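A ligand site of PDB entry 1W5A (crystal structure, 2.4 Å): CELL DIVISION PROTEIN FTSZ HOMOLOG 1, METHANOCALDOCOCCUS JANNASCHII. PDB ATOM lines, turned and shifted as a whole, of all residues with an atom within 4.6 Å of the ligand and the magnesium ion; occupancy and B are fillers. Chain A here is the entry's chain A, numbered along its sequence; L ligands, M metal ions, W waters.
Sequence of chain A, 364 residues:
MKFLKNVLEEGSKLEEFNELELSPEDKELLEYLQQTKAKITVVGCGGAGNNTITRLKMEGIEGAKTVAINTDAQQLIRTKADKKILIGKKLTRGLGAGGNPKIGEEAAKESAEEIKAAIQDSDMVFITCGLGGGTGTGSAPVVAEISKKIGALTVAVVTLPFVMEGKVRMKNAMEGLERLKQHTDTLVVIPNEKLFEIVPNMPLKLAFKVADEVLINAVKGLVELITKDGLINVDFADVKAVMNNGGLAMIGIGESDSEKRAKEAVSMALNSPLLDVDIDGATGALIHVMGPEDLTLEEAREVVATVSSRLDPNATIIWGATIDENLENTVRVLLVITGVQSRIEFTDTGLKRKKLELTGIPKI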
ATOM      1  N   CYS A  45     -14.281  -5.725   6.103  1.00  0.00           N
ATOM      2  CA  CYS A  45     -13.797  -6.335   4.863  1.00  0.00           C
ATOM      3  C   CYS A  45     -13.524  -7.820   5.030  1.00  0.00           C
ATOM      4  O   CYS A  45     -12.990  -8.242   6.056  1.00  0.00           O
ATOM      5  CB  CYS A  45     -12.511  -5.651   4.399  1.00  0.00           C
ATOM      6  SG  CYS A  45     -12.573  -3.847   4.492  1.00  0.00           S
ATOM      7  N   GLY A  46     -13.866  -8.617   4.021  1.00  0.00           N
ATOM      8  CA  GLY A  46     -13.645 -10.052   4.117  1.00  0.00           C
ATOM      9  C   GLY A  46     -14.681 -10.741   5.010  1.00  0.00           C
ATOM     10  O   GLY A  46     -15.568 -10.088   5.582  1.00  0.00           O
ATOM     11  N   GLY A  47     -14.554 -12.063   5.125  1.00  0.00           N
ATOM     12  CA  GLY A  47     -15.469 -12.832   5.943  1.00  0.00           C
ATOM     13  C   GLY A  47     -15.513 -12.388   7.400  1.00  0.00           C
ATOM     14  O   GLY A  47     -16.578 -12.044   7.922  1.00  0.00           O
ATOM     15  N   ALA A  48     -14.371 -12.421   8.068  1.00  0.00           N
ATOM     16  CA  ALA A  48     -14.313 -12.002   9.472  1.00  0.00           C
ATOM     17  C   ALA A  48     -14.927 -10.604   9.566  1.00  0.00           C
ATOM     18  O   ALA A  48     -15.789 -10.339  10.402  1.00  0.00           O
ATOM     19  CB  ALA A  48     -12.860 -11.987   9.967  1.00  0.00           C
ATOM     20  N   GLY A  49     -14.475  -9.700   8.690  1.00  0.00           N
ATOM     21  CA  GLY A  49     -15.014  -8.357   8.701  1.00  0.00           C
ATOM     22  C   GLY A  49     -16.522  -8.329   8.517  1.00  0.00           C
ATOM     23  O   GLY A  49     -17.223  -7.601   9.209  1.00  0.00           O
ATOM     24  N   ASN A  51     -18.651 -10.796   9.114  1.00  0.00           N
ATOM     25  CA  ASN A  51     -19.297 -11.425  10.266  1.00  0.00           C
ATOM     26  C   ASN A  51     -19.413 -10.427  11.407  1.00  0.00           C
ATOM     27  O   ASN A  51     -20.369 -10.460  12.176  1.00  0.00           O
ATOM     28  CB  ASN A  51     -18.513 -12.666  10.719  1.00  0.00           C
ATOM     29  CG  ASN A  51     -19.139 -13.343  11.940  1.00  0.00           C
ATOM     30  OD1 ASN A  51     -20.328 -13.648  11.956  1.00  0.00           O
ATOM     31  ND2 ASN A  51     -18.320 -13.582  12.959  1.00  0.00           N
ATOM     32  N   ASN A  70     -16.781  -7.409   0.227  1.00  0.00           N
ATOM     33  CA  ASN A  70     -16.128  -8.685   0.060  1.00  0.00           C
ATOM     34  C   ASN A  70     -16.059  -9.036  -1.419  1.00  0.00           C
ATOM     35  O   ASN A  70     -16.716  -8.415  -2.254  1.00  0.00           O
ATOM     36  CB  ASN A  70     -16.921  -9.743   0.846  1.00  0.00           C
ATOM     37  CG  ASN A  70     -16.075 -10.939   1.242  1.00  0.00           C
ATOM     38  OD1 ASN A  70     -16.422 -11.643   2.195  1.00  0.00           O
ATOM     39  ND2 ASN A  70     -14.993 -11.201   0.513  1.00  0.00           N
ATOM     40  N   THR A  71     -15.215 -10.002  -1.742  1.00  0.00           N
ATOM     41  CA  THR A  71     -15.084 -10.485  -3.104  1.00  0.00           C
ATOM     42  C   THR A  71     -16.009 -11.715  -3.205  1.00  0.00           C
ATOM     43  O   THR A  71     -16.583 -11.996  -4.266  1.00  0.00           O
ATOM     44  CB  THR A  71     -13.635 -10.915  -3.391  1.00  0.00           C
ATOM     45  OG1 THR A  71     -13.129 -11.663  -2.277  1.00  0.00           O
ATOM     46  CG2 THR A  71     -12.766  -9.692  -3.608  1.00  0.00           C
ATOM     47  N   ASP A  72     -16.159 -12.426  -2.086  1.00  0.00           N
ATOM     48  CA  ASP A  72     -16.990 -13.627  -1.987  1.00  0.00           C
ATOM     49  C   ASP A  72     -18.462 -13.217  -1.911  1.00  0.00           C
ATOM     50  O   ASP A  72     -18.930 -12.817  -0.845  1.00  0.00           O
ATOM     51  CB  ASP A  72     -16.600 -14.422  -0.732  1.00  0.00           C
ATOM     52  CG  ASP A  72     -17.240 -15.799  -0.680  1.00  0.00           C
ATOM     53  OD1 ASP A  72     -18.417 -15.950  -1.082  1.00  0.00           O
ATOM     54  OD2 ASP A  72     -16.548 -16.732  -0.207  1.00  0.00           O
ATOM     55  N   GLN A  75     -20.514 -15.069   0.887  1.00  0.00           N
ATOM     56  CA  GLN A  75     -20.385 -14.572   2.258  1.00  0.00           C
ATOM     57  C   GLN A  75     -21.144 -13.264   2.405  1.00  0.00           C
ATOM     58  O   GLN A  75     -21.807 -13.026   3.421  1.00  0.00           O
ATOM     59  CB  GLN A  75     -18.919 -14.318   2.634  1.00  0.00           C
ATOM     60  CG  GLN A  75     -18.031 -15.548   2.643  1.00  0.00           C
ATOM     61  CD  GLN A  75     -16.656 -15.251   3.224  1.00  0.00           C
ATOM     62  OE1 GLN A  75     -15.979 -14.318   2.799  1.00  0.00           O
ATOM     63  NE2 GLN A  75     -16.239 -16.052   4.203  1.00  0.00           N
ATOM     64  N   GLY A  96     -13.999 -15.568  -3.596  1.00  0.00           N
ATOM     65  CA  GLY A  96     -13.031 -15.038  -2.653  1.00  0.00           C
ATOM     66  C   GLY A  96     -11.672 -14.885  -3.310  1.00  0.00           C
ATOM     67  O   GLY A  96     -11.507 -15.178  -4.498  1.00  0.00           O
ATOM     68  N   ALA A  97     -10.691 -14.435  -2.530  1.00  0.00           N
ATOM     69  CA  ALA A  97      -9.336 -14.221  -3.030  1.00  0.00           C
ATOM     70  C   ALA A  97      -8.416 -15.417  -2.774  1.00  0.00           C
ATOM     71  O   ALA A  97      -7.234 -15.379  -3.132  1.00  0.00           O
ATOM     72  CB  ALA A  97      -8.741 -12.961  -2.385  1.00  0.00           C
ATOM     73  N   GLY A  98      -8.958 -16.463  -2.160  1.00  0.00           N
ATOM     74  CA  GLY A  98      -8.163 -17.651  -1.884  1.00  0.00           C
ATOM     75  C   GLY A  98      -6.912 -17.405  -1.054  1.00  0.00           C
ATOM     76  O   GLY A  98      -5.936 -18.152  -1.188  1.00  0.00           O
ATOM     77  N   GLY A  99      -6.919 -16.373  -0.216  1.00  0.00           N
ATOM     78  CA  GLY A  99      -5.760 -16.077   0.623  1.00  0.00           C
ATOM     79  C   GLY A  99      -4.705 -15.202  -0.029  1.00  0.00           C
ATOM     80  O   GLY A  99      -3.631 -14.967   0.547  1.00  0.00           O
ATOM     81  N   ASN A 100      -4.996 -14.698  -1.229  1.00  0.00           N
ATOM     82  CA  ASN A 100      -4.058 -13.862  -1.960  1.00  0.00           C
ATOM     83  C   ASN A 100      -4.305 -12.368  -1.672  1.00  0.00           C
ATOM     84  O   ASN A 100      -5.192 -11.758  -2.273  1.00  0.00           O
ATOM     85  CB  ASN A 100      -4.200 -14.135  -3.446  1.00  0.00           C
ATOM     86  CG  ASN A 100      -3.089 -13.514  -4.254  1.00  0.00           C
ATOM     87  OD1 ASN A 100      -2.754 -12.340  -4.083  1.00  0.00           O
ATOM     88  ND2 ASN A 100      -2.511 -14.297  -5.162  1.00  0.00           N
ATOM     89  N   GLY A 130     -10.228  -9.336   9.680  1.00  0.00           N
ATOM     90  CA  GLY A 130      -9.310 -10.257  10.306  1.00  0.00           C
ATOM     91  C   GLY A 130      -8.153 -10.300   9.313  1.00  0.00           C
ATOM     92  O   GLY A 130      -8.369 -10.656   8.157  1.00  0.00           O
ATOM     93  N   LEU A 131      -6.961  -9.917   9.731  1.00  0.00           N
ATOM     94  CA  LEU A 131      -5.829  -9.944   8.811  1.00  0.00           C
ATOM     95  C   LEU A 131      -5.368 -11.388   8.668  1.00  0.00           C
ATOM     96  O   LEU A 131      -5.483 -12.167   9.603  1.00  0.00           O
ATOM     97  CB  LEU A 131      -4.704  -9.060   9.335  1.00  0.00           C
ATOM     98  CG  LEU A 131      -4.996  -7.564   9.514  1.00  0.00           C
ATOM     99  CD1 LEU A 131      -3.803  -6.862  10.141  1.00  0.00           C
ATOM    100  CD2 LEU A 131      -5.332  -6.956   8.166  1.00  0.00           C
ATOM    101  N   GLY A 132      -4.853 -11.750   7.497  1.00  0.00           N
ATOM    102  CA  GLY A 132      -4.386 -13.112   7.291  1.00  0.00           C
ATOM    103  C   GLY A 132      -4.942 -13.733   6.018  1.00  0.00           C
ATOM    104  O   GLY A 132      -4.351 -14.645   5.443  1.00  0.00           O
ATOM    105  N   GLY A 133      -6.114 -13.261   5.588  1.00  0.00           N
ATOM    106  CA  GLY A 133      -6.721 -13.793   4.379  1.00  0.00           C
ATOM    107  C   GLY A 133      -6.304 -12.971   3.178  1.00  0.00           C
ATOM    108  O   GLY A 133      -5.314 -12.234   3.240  1.00  0.00           O
ATOM    109  N   GLY A 134      -7.036 -13.084   2.074  1.00  0.00           N
ATOM    110  CA  GLY A 134      -6.691 -12.312   0.897  1.00  0.00           C
ATOM    111  C   GLY A 134      -7.464 -11.014   0.731  1.00  0.00           C
ATOM    112  O   GLY A 134      -6.915  -9.983   0.350  1.00  0.00           O
ATOM    113  N   THR A 135      -8.761 -11.045   1.051  1.00  0.00           N
ATOM    114  CA  THR A 135      -9.594  -9.871   0.899  1.00  0.00           C
ATOM    115  C   THR A 135      -9.397  -8.812   1.987  1.00  0.00           C
ATOM    116  O   THR A 135      -9.084  -7.652   1.691  1.00  0.00           O
ATOM    117  CB  THR A 135     -11.057 -10.284   0.870  1.00  0.00           C
ATOM    118  OG1 THR A 135     -11.220 -11.341  -0.076  1.00  0.00           O
ATOM    119  CG2 THR A 135     -11.921  -9.111   0.453  1.00  0.00           C
ATOM    120  N   GLY A 136      -9.585  -9.202   3.247  1.00  0.00           N
ATOM    121  CA  GLY A 136      -9.422  -8.261   4.339  1.00  0.00           C
ATOM    122  C   GLY A 136      -8.045  -7.638   4.297  1.00  0.00           C
ATOM    123  O   GLY A 136      -7.904  -6.415   4.229  1.00  0.00           O
ATOM    124  N   PRO A 161      -3.954 -13.392  13.158  1.00  0.00           N
ATOM    125  CA  PRO A 161      -4.362 -14.796  13.269  1.00  0.00           C
ATOM    126  C   PRO A 161      -3.738 -15.605  14.417  1.00  0.00           C
ATOM    127  O   PRO A 161      -2.719 -15.207  14.985  1.00  0.00           O
ATOM    128  CB  PRO A 161      -3.988 -15.366  11.911  1.00  0.00           C
ATOM    129  CG  PRO A 161      -2.688 -14.616  11.617  1.00  0.00           C
ATOM    130  CD  PRO A 161      -3.010 -13.189  12.042  1.00  0.00           C
ATOM    131  N   GLU A 165      -2.877 -21.177  12.699  1.00  0.00           N
ATOM    132  CA  GLU A 165      -3.280 -20.933  11.322  1.00  0.00           C
ATOM    133  C   GLU A 165      -2.108 -20.993  10.340  1.00  0.00           C
ATOM    134  O   GLU A 165      -2.307 -20.884   9.133  1.00  0.00           O
ATOM    135  CB  GLU A 165      -3.987 -19.579  11.183  1.00  0.00           C
ATOM    136  CG  GLU A 165      -5.329 -19.504  11.905  1.00  0.00           C
ATOM    137  CD  GLU A 165      -6.104 -18.225  11.590  1.00  0.00           C
ATOM    138  OE1 GLU A 165      -6.566 -18.076  10.442  1.00  0.00           O
ATOM    139  OE2 GLU A 165      -6.254 -17.371  12.494  1.00  0.00           O
ATOM    140  N   ARG A 169      -0.144 -17.358   6.973  1.00  0.00           N
ATOM    141  CA  ARG A 169      -1.243 -16.447   7.341  1.00  0.00           C
ATOM    142  C   ARG A 169      -0.760 -15.268   8.187  1.00  0.00           C
ATOM    143  O   ARG A 169      -1.219 -14.137   8.027  1.00  0.00           O
ATOM    144  CB  ARG A 169      -2.336 -17.215   8.086  1.00  0.00           C
ATOM    145  CG  ARG A 169      -3.716 -16.990   7.514  1.00  0.00           C
ATOM    146  CD  ARG A 169      -4.308 -18.239   6.951  1.00  0.00           C
ATOM    147  NE  ARG A 169      -5.011 -18.044   5.688  1.00  0.00           N
ATOM    148  CZ  ARG A 169      -6.167 -17.398   5.502  1.00  0.00           C
ATOM    149  NH1 ARG A 169      -6.822 -16.825   6.515  1.00  0.00           N
ATOM    150  NH2 ARG A 169      -6.686 -17.348   4.282  1.00  0.00           N
ATOM    151  N   ASN A 192      -5.117 -12.438  18.215  1.00  0.00           N
ATOM    152  CA  ASN A 192      -5.963 -13.562  18.563  1.00  0.00           C
ATOM    153  C   ASN A 192      -5.268 -14.605  19.436  1.00  0.00           C
ATOM    154  O   ASN A 192      -5.885 -15.155  20.348  1.00  0.00           O
ATOM    155  CB  ASN A 192      -6.499 -14.223  17.302  1.00  0.00           C
ATOM    156  CG  ASN A 192      -7.741 -13.540  16.759  1.00  0.00           C
ATOM    157  OD1 ASN A 192      -8.180 -13.805  15.634  1.00  0.00           O
ATOM    158  ND2 ASN A 192      -8.338 -12.664  17.561  1.00  0.00           N
ATOM    159  N   PHE A 208     -12.691 -18.940  17.317  1.00  0.00           N
ATOM    160  CA  PHE A 208     -13.228 -17.817  16.553  1.00  0.00           C
ATOM    161  C   PHE A 208     -14.500 -17.220  17.145  1.00  0.00           C
ATOM    162  O   PHE A 208     -14.805 -16.049  16.882  1.00  0.00           O
ATOM    163  CB  PHE A 208     -13.418 -18.234  15.099  1.00  0.00           C
ATOM    164  CG  PHE A 208     -12.134 -18.505  14.375  1.00  0.00           C
ATOM    165  CD1 PHE A 208     -11.166 -17.506  14.276  1.00  0.00           C
ATOM    166  CD2 PHE A 208     -11.863 -19.759  13.824  1.00  0.00           C
ATOM    167  CE1 PHE A 208      -9.941 -17.747  13.641  1.00  0.00           C
ATOM    168  CE2 PHE A 208     -10.648 -20.016  13.175  1.00  0.00           C
ATOM    169  CZ  PHE A 208      -9.680 -19.008  13.081  1.00  0.00           C
ATOM    170  N   ALA A 211     -13.020 -14.823  19.592  1.00  0.00           N
ATOM    171  CA  ALA A 211     -12.429 -13.683  18.894  1.00  0.00           C
ATOM    172  C   ALA A 211     -13.557 -12.740  18.404  1.00  0.00           C
ATOM    173  O   ALA A 211     -13.427 -11.509  18.485  1.00  0.00           O
ATOM    174  CB  ALA A 211     -11.598 -14.178  17.711  1.00  0.00           C
ATOM    175  N   ASP A 212     -14.652 -13.323  17.918  1.00  0.00           N
ATOM    176  CA  ASP A 212     -15.781 -12.519  17.449  1.00  0.00           C
ATOM    177  C   ASP A 212     -16.232 -11.572  18.562  1.00  0.00           C
ATOM    178  O   ASP A 212     -16.500 -10.391  18.323  1.00  0.00           O
ATOM    179  CB  ASP A 212     -16.971 -13.404  17.069  1.00  0.00           C
ATOM    180  CG  ASP A 212     -16.806 -14.071  15.730  1.00  0.00           C
ATOM    181  OD1 ASP A 212     -15.869 -13.716  14.997  1.00  0.00           O
ATOM    182  OD2 ASP A 212     -17.626 -14.955  15.404  1.00  0.00           O
ATOM    183  N   LEU A 215     -13.632  -8.774  19.180  1.00  0.00           N
ATOM    184  CA  LEU A 215     -13.740  -7.822  18.087  1.00  0.00           C
ATOM    185  C   LEU A 215     -14.968  -6.936  18.267  1.00  0.00           C
ATOM    186  O   LEU A 215     -14.870  -5.717  18.225  1.00  0.00           O
ATOM    187  CB  LEU A 215     -13.837  -8.553  16.748  1.00  0.00           C
ATOM    188  CG  LEU A 215     -12.568  -8.630  15.902  1.00  0.00           C
ATOM    189  CD1 LEU A 215     -12.811  -9.575  14.732  1.00  0.00           C
ATOM    190  CD2 LEU A 215     -12.202  -7.231  15.407  1.00  0.00           C
HETATM  191  P1  LIG L   1     -10.236 -14.522   1.435  1.00  0.00           P
HETATM  192  O1  LIG L   1      -8.829 -15.085   1.139  1.00  0.00           O
HETATM  193  O2  LIG L   1     -11.199 -15.647   1.863  1.00  0.00           O
HETATM  194  O3  LIG L   1     -10.837 -13.897   0.167  1.00  0.00           O
HETATM  195  O4  LIG L   1     -10.068 -13.347   2.601  1.00  0.00           O
HETATM  196  P2  LIG L   1     -11.028 -12.952   3.876  1.00  0.00           P
HETATM  197  O5  LIG L   1     -12.453 -13.160   3.584  1.00  0.00           O
HETATM  198  O6  LIG L   1     -10.598 -11.546   4.252  1.00  0.00           O
HETATM  199  O7  LIG L   1     -10.634 -13.896   5.049  1.00  0.00           O
HETATM  200  P3  LIG L   1     -11.292 -14.182   6.429  1.00  0.00           P
HETATM  201  O8  LIG L   1     -12.098 -15.432   6.349  1.00  0.00           O
HETATM  202  O9  LIG L   1     -11.896 -12.981   6.977  1.00  0.00           O
HETATM  203  O10 LIG L   1      -9.958 -14.640   7.270  1.00  0.00           O
HETATM  204  C1  LIG L   1      -8.997 -13.721   7.785  1.00  0.00           C
HETATM  205  C2  LIG L   1      -8.631 -14.072   9.208  1.00  0.00           C
HETATM  206  O11 LIG L   1      -9.757 -13.799  10.059  1.00  0.00           O
HETATM  207  C3  LIG L   1      -8.297 -15.558   9.441  1.00  0.00           C
HETATM  208  O12 LIG L   1      -6.913 -15.773   9.259  1.00  0.00           O
HETATM  209  C4  LIG L   1      -8.660 -15.751  10.917  1.00  0.00           C
HETATM  210  O13 LIG L   1      -7.626 -15.231  11.737  1.00  0.00           O
HETATM  211  C5  LIG L   1      -9.844 -14.784  11.077  1.00  0.00           C
HETATM  212  N1  LIG L   1     -11.174 -15.405  11.055  1.00  0.00           N
HETATM  213  C6  LIG L   1     -11.744 -16.138  10.024  1.00  0.00           C
HETATM  214  N2  LIG L   1     -12.939 -16.583  10.331  1.00  0.00           N
HETATM  215  C7  LIG L   1     -13.299 -15.822  11.430  1.00  0.00           C
HETATM  216  C8  LIG L   1     -14.526 -15.613  12.084  1.00  0.00           C
HETATM  217  O14 LIG L   1     -15.626 -16.092  11.780  1.00  0.00           O
HETATM  218  N3  LIG L   1     -14.428 -14.720  13.155  1.00  0.00           N
HETATM  219  C9  LIG L   1     -13.284 -14.016  13.509  1.00  0.00           C
HETATM  220  N4  LIG L   1     -13.357 -13.217  14.556  1.00  0.00           N
HETATM  221  N5  LIG L   1     -12.121 -14.217  12.942  1.00  0.00           N
HETATM  222  C10 LIG L   1     -12.195 -15.050  11.867  1.00  0.00           C
HETATM  223 MG    MG M   1     -13.363 -14.953   1.644  1.00  0.00          MG
HETATM  224  O   HOH W   1     -15.903 -12.004  12.778  1.00  0.00           O
HETATM  225  O   HOH W   2     -11.241 -17.192  -0.766  1.00  0.00           O
HETATM  226  O   HOH W   3     -13.353 -15.888   3.786  1.00  0.00           O
HETATM  227  O   HOH W   4     -13.540 -13.249   0.638  1.00  0.00           O
HETATM  228  O   HOH W   5     -14.283 -16.915   7.459  1.00  0.00           O
HETATM  229  O   HOH W   6      -8.185 -11.058   5.567  1.00  0.00           O
HETATM  230  O   HOH W   7     -17.184 -17.007  13.891  1.00  0.00           O
HETATM  231  O   HOH W   8     -11.798 -10.211   7.461  1.00  0.00           O
HETATM  232  O   HOH W   9     -13.943 -16.712   0.745  1.00  0.00           O
HETATM  233  O   HOH W  10     -10.373 -12.491  14.409  1.00  0.00           O
HETATM  234  O   HOH W  11      -7.014 -12.538  11.851  1.00  0.00           O
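Merely in contact with the magnesium ion: Gln 75.
Of the 30 residues printed, 1 comes within 4 Å of the magnesium ion.
Merely in contact with the ligand: Gly 130 (3.2 Å), Gly 46 (3.4 Å), Gly 98 (3.6 Å), Phe 208 (3.6 Å), Pro 161 (3.6 Å), Gly 133 (3.7 Å), Leu 215 (3.7 Å), Leu 131 (3.7 Å), Gly 96 (3.7 Å), Ala 211 (3.7 Å), Gln 75 (3.8 Å) and Asn 51 (3.9 Å).
Hydrophobic or aromatic side chains that line the ligand: Ala 48, Ala 97, Pro 161, Phe 208, Ala 211 and Leu 215.
The nearest printed residue that does not touch the ligand is Thr 71 (4.03 Å).
Water W4 lies within hydrogen-bond range of ND2 of Asn 70 (2.5 Å), O3 of the ligand (2.8 Å), OG1 of Thr 135 (3.1 Å), OG1 of Thr 71 (3.3 Å) and OE1 of Gln 75 (3.4 Å).
Water W11 bridges O of Leu 131 (2.7 Å) and O13 of the ligand (2.8 Å).
Water W7 bridges OD2 of Asp 212 (2.6 Å) and O14 of the ligand (2.8 Å).
Water W6 lies within hydrogen-bond range of O of Gly 130 (2.6 Å), O6 of the ligand (2.8 Å), N of Gly 133 (3.0 Å) and N of Gly 136 (3.3 Å).
Water W10 lies within hydrogen-bond range of the side-chain amide oxygen (OD1) of Asn 192 (2.8 Å) and a nitrogen (N5) of the ligand (2.9 Å).
Water W2 lies within hydrogen-bond range of N of Gly 98, N of Ala 97 and O3 of the ligand.
Water W4 binds the magnesium ion (2.0 Å).
The magnesium ion is bound by water W9 (2.1 Å).
The magnesium ion is bound by O2 of the ligand, 2.3 Å away.
The magnesium ion is bound by water W3, at 2.3 Å.
Slightly farther from the magnesium ion lies an oxygen (O5) of the ligand (2.8 Å).
A nitrogen (N3) of the ligand lies within hydrogen-bond range of the side-chain carboxylate (OD1) of Asp 212, at 2.5 Å.
The backbone NH (N) of Thr 135 sits at hydrogen-bond distance from an oxygen (O4) of the ligand, at 3.1 Å.
OG1 of Thr 135 is in hydrogen-bond range of O3 of the ligand.
The side-chain carboxylate (OE1) of Glu 165 is in hydrogen-bond range of an oxygen (O12) of the ligand (2.6 Å).
O1 of the ligand sits at hydrogen-bond distance from N of Gly 99 (2.7 Å).
O6 of the ligand lies within hydrogen-bond range of N of Gly 136.
The backbone NH (N) of Ala 97 is in hydrogen-bond range of an oxygen (O3) of the ligand (2.8 Å).
O9 of the ligand sits at hydrogen-bond distance from N of Ala 48, at 2.8 Å.
The backbone NH (N) of Gly 47 lies within hydrogen-bond range of an oxygen (O5) of the ligand (2.8 Å).
The backbone NH (N) of Gly 134 lies within hydrogen-bond range of an oxygen (O1) of the ligand.
NH1 of Arg 169 lies within hydrogen-bond range of O12 of the ligand (2.9 Å).
The side-chain carboxylate (OD2) of Asp 212 lies within hydrogen-bond range of the side-chain amide nitrogen (ND2) of Asn 51 (2.9 Å).
The side-chain hydroxyl of Thr 71 is in hydrogen-bond range of the side-chain hydroxyl of Thr 135.
N of Gly 47 lies within hydrogen-bond range of OD1 of Asn 70, 3.5 Å away.
N of Gln 75 sits at hydrogen-bond distance from OD1 of Asp 72 (3.0 Å).
The side-chain amide oxygen (OE1) of Gln 75 lies close to the side-chain amide oxygen (OD1) of Asn 70, at 2.8 Å.
The guanidinium group (NH1) of Arg 169 lies close to the backbone carbonyl oxygen (O) of Gly 132 (3.5 Å).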
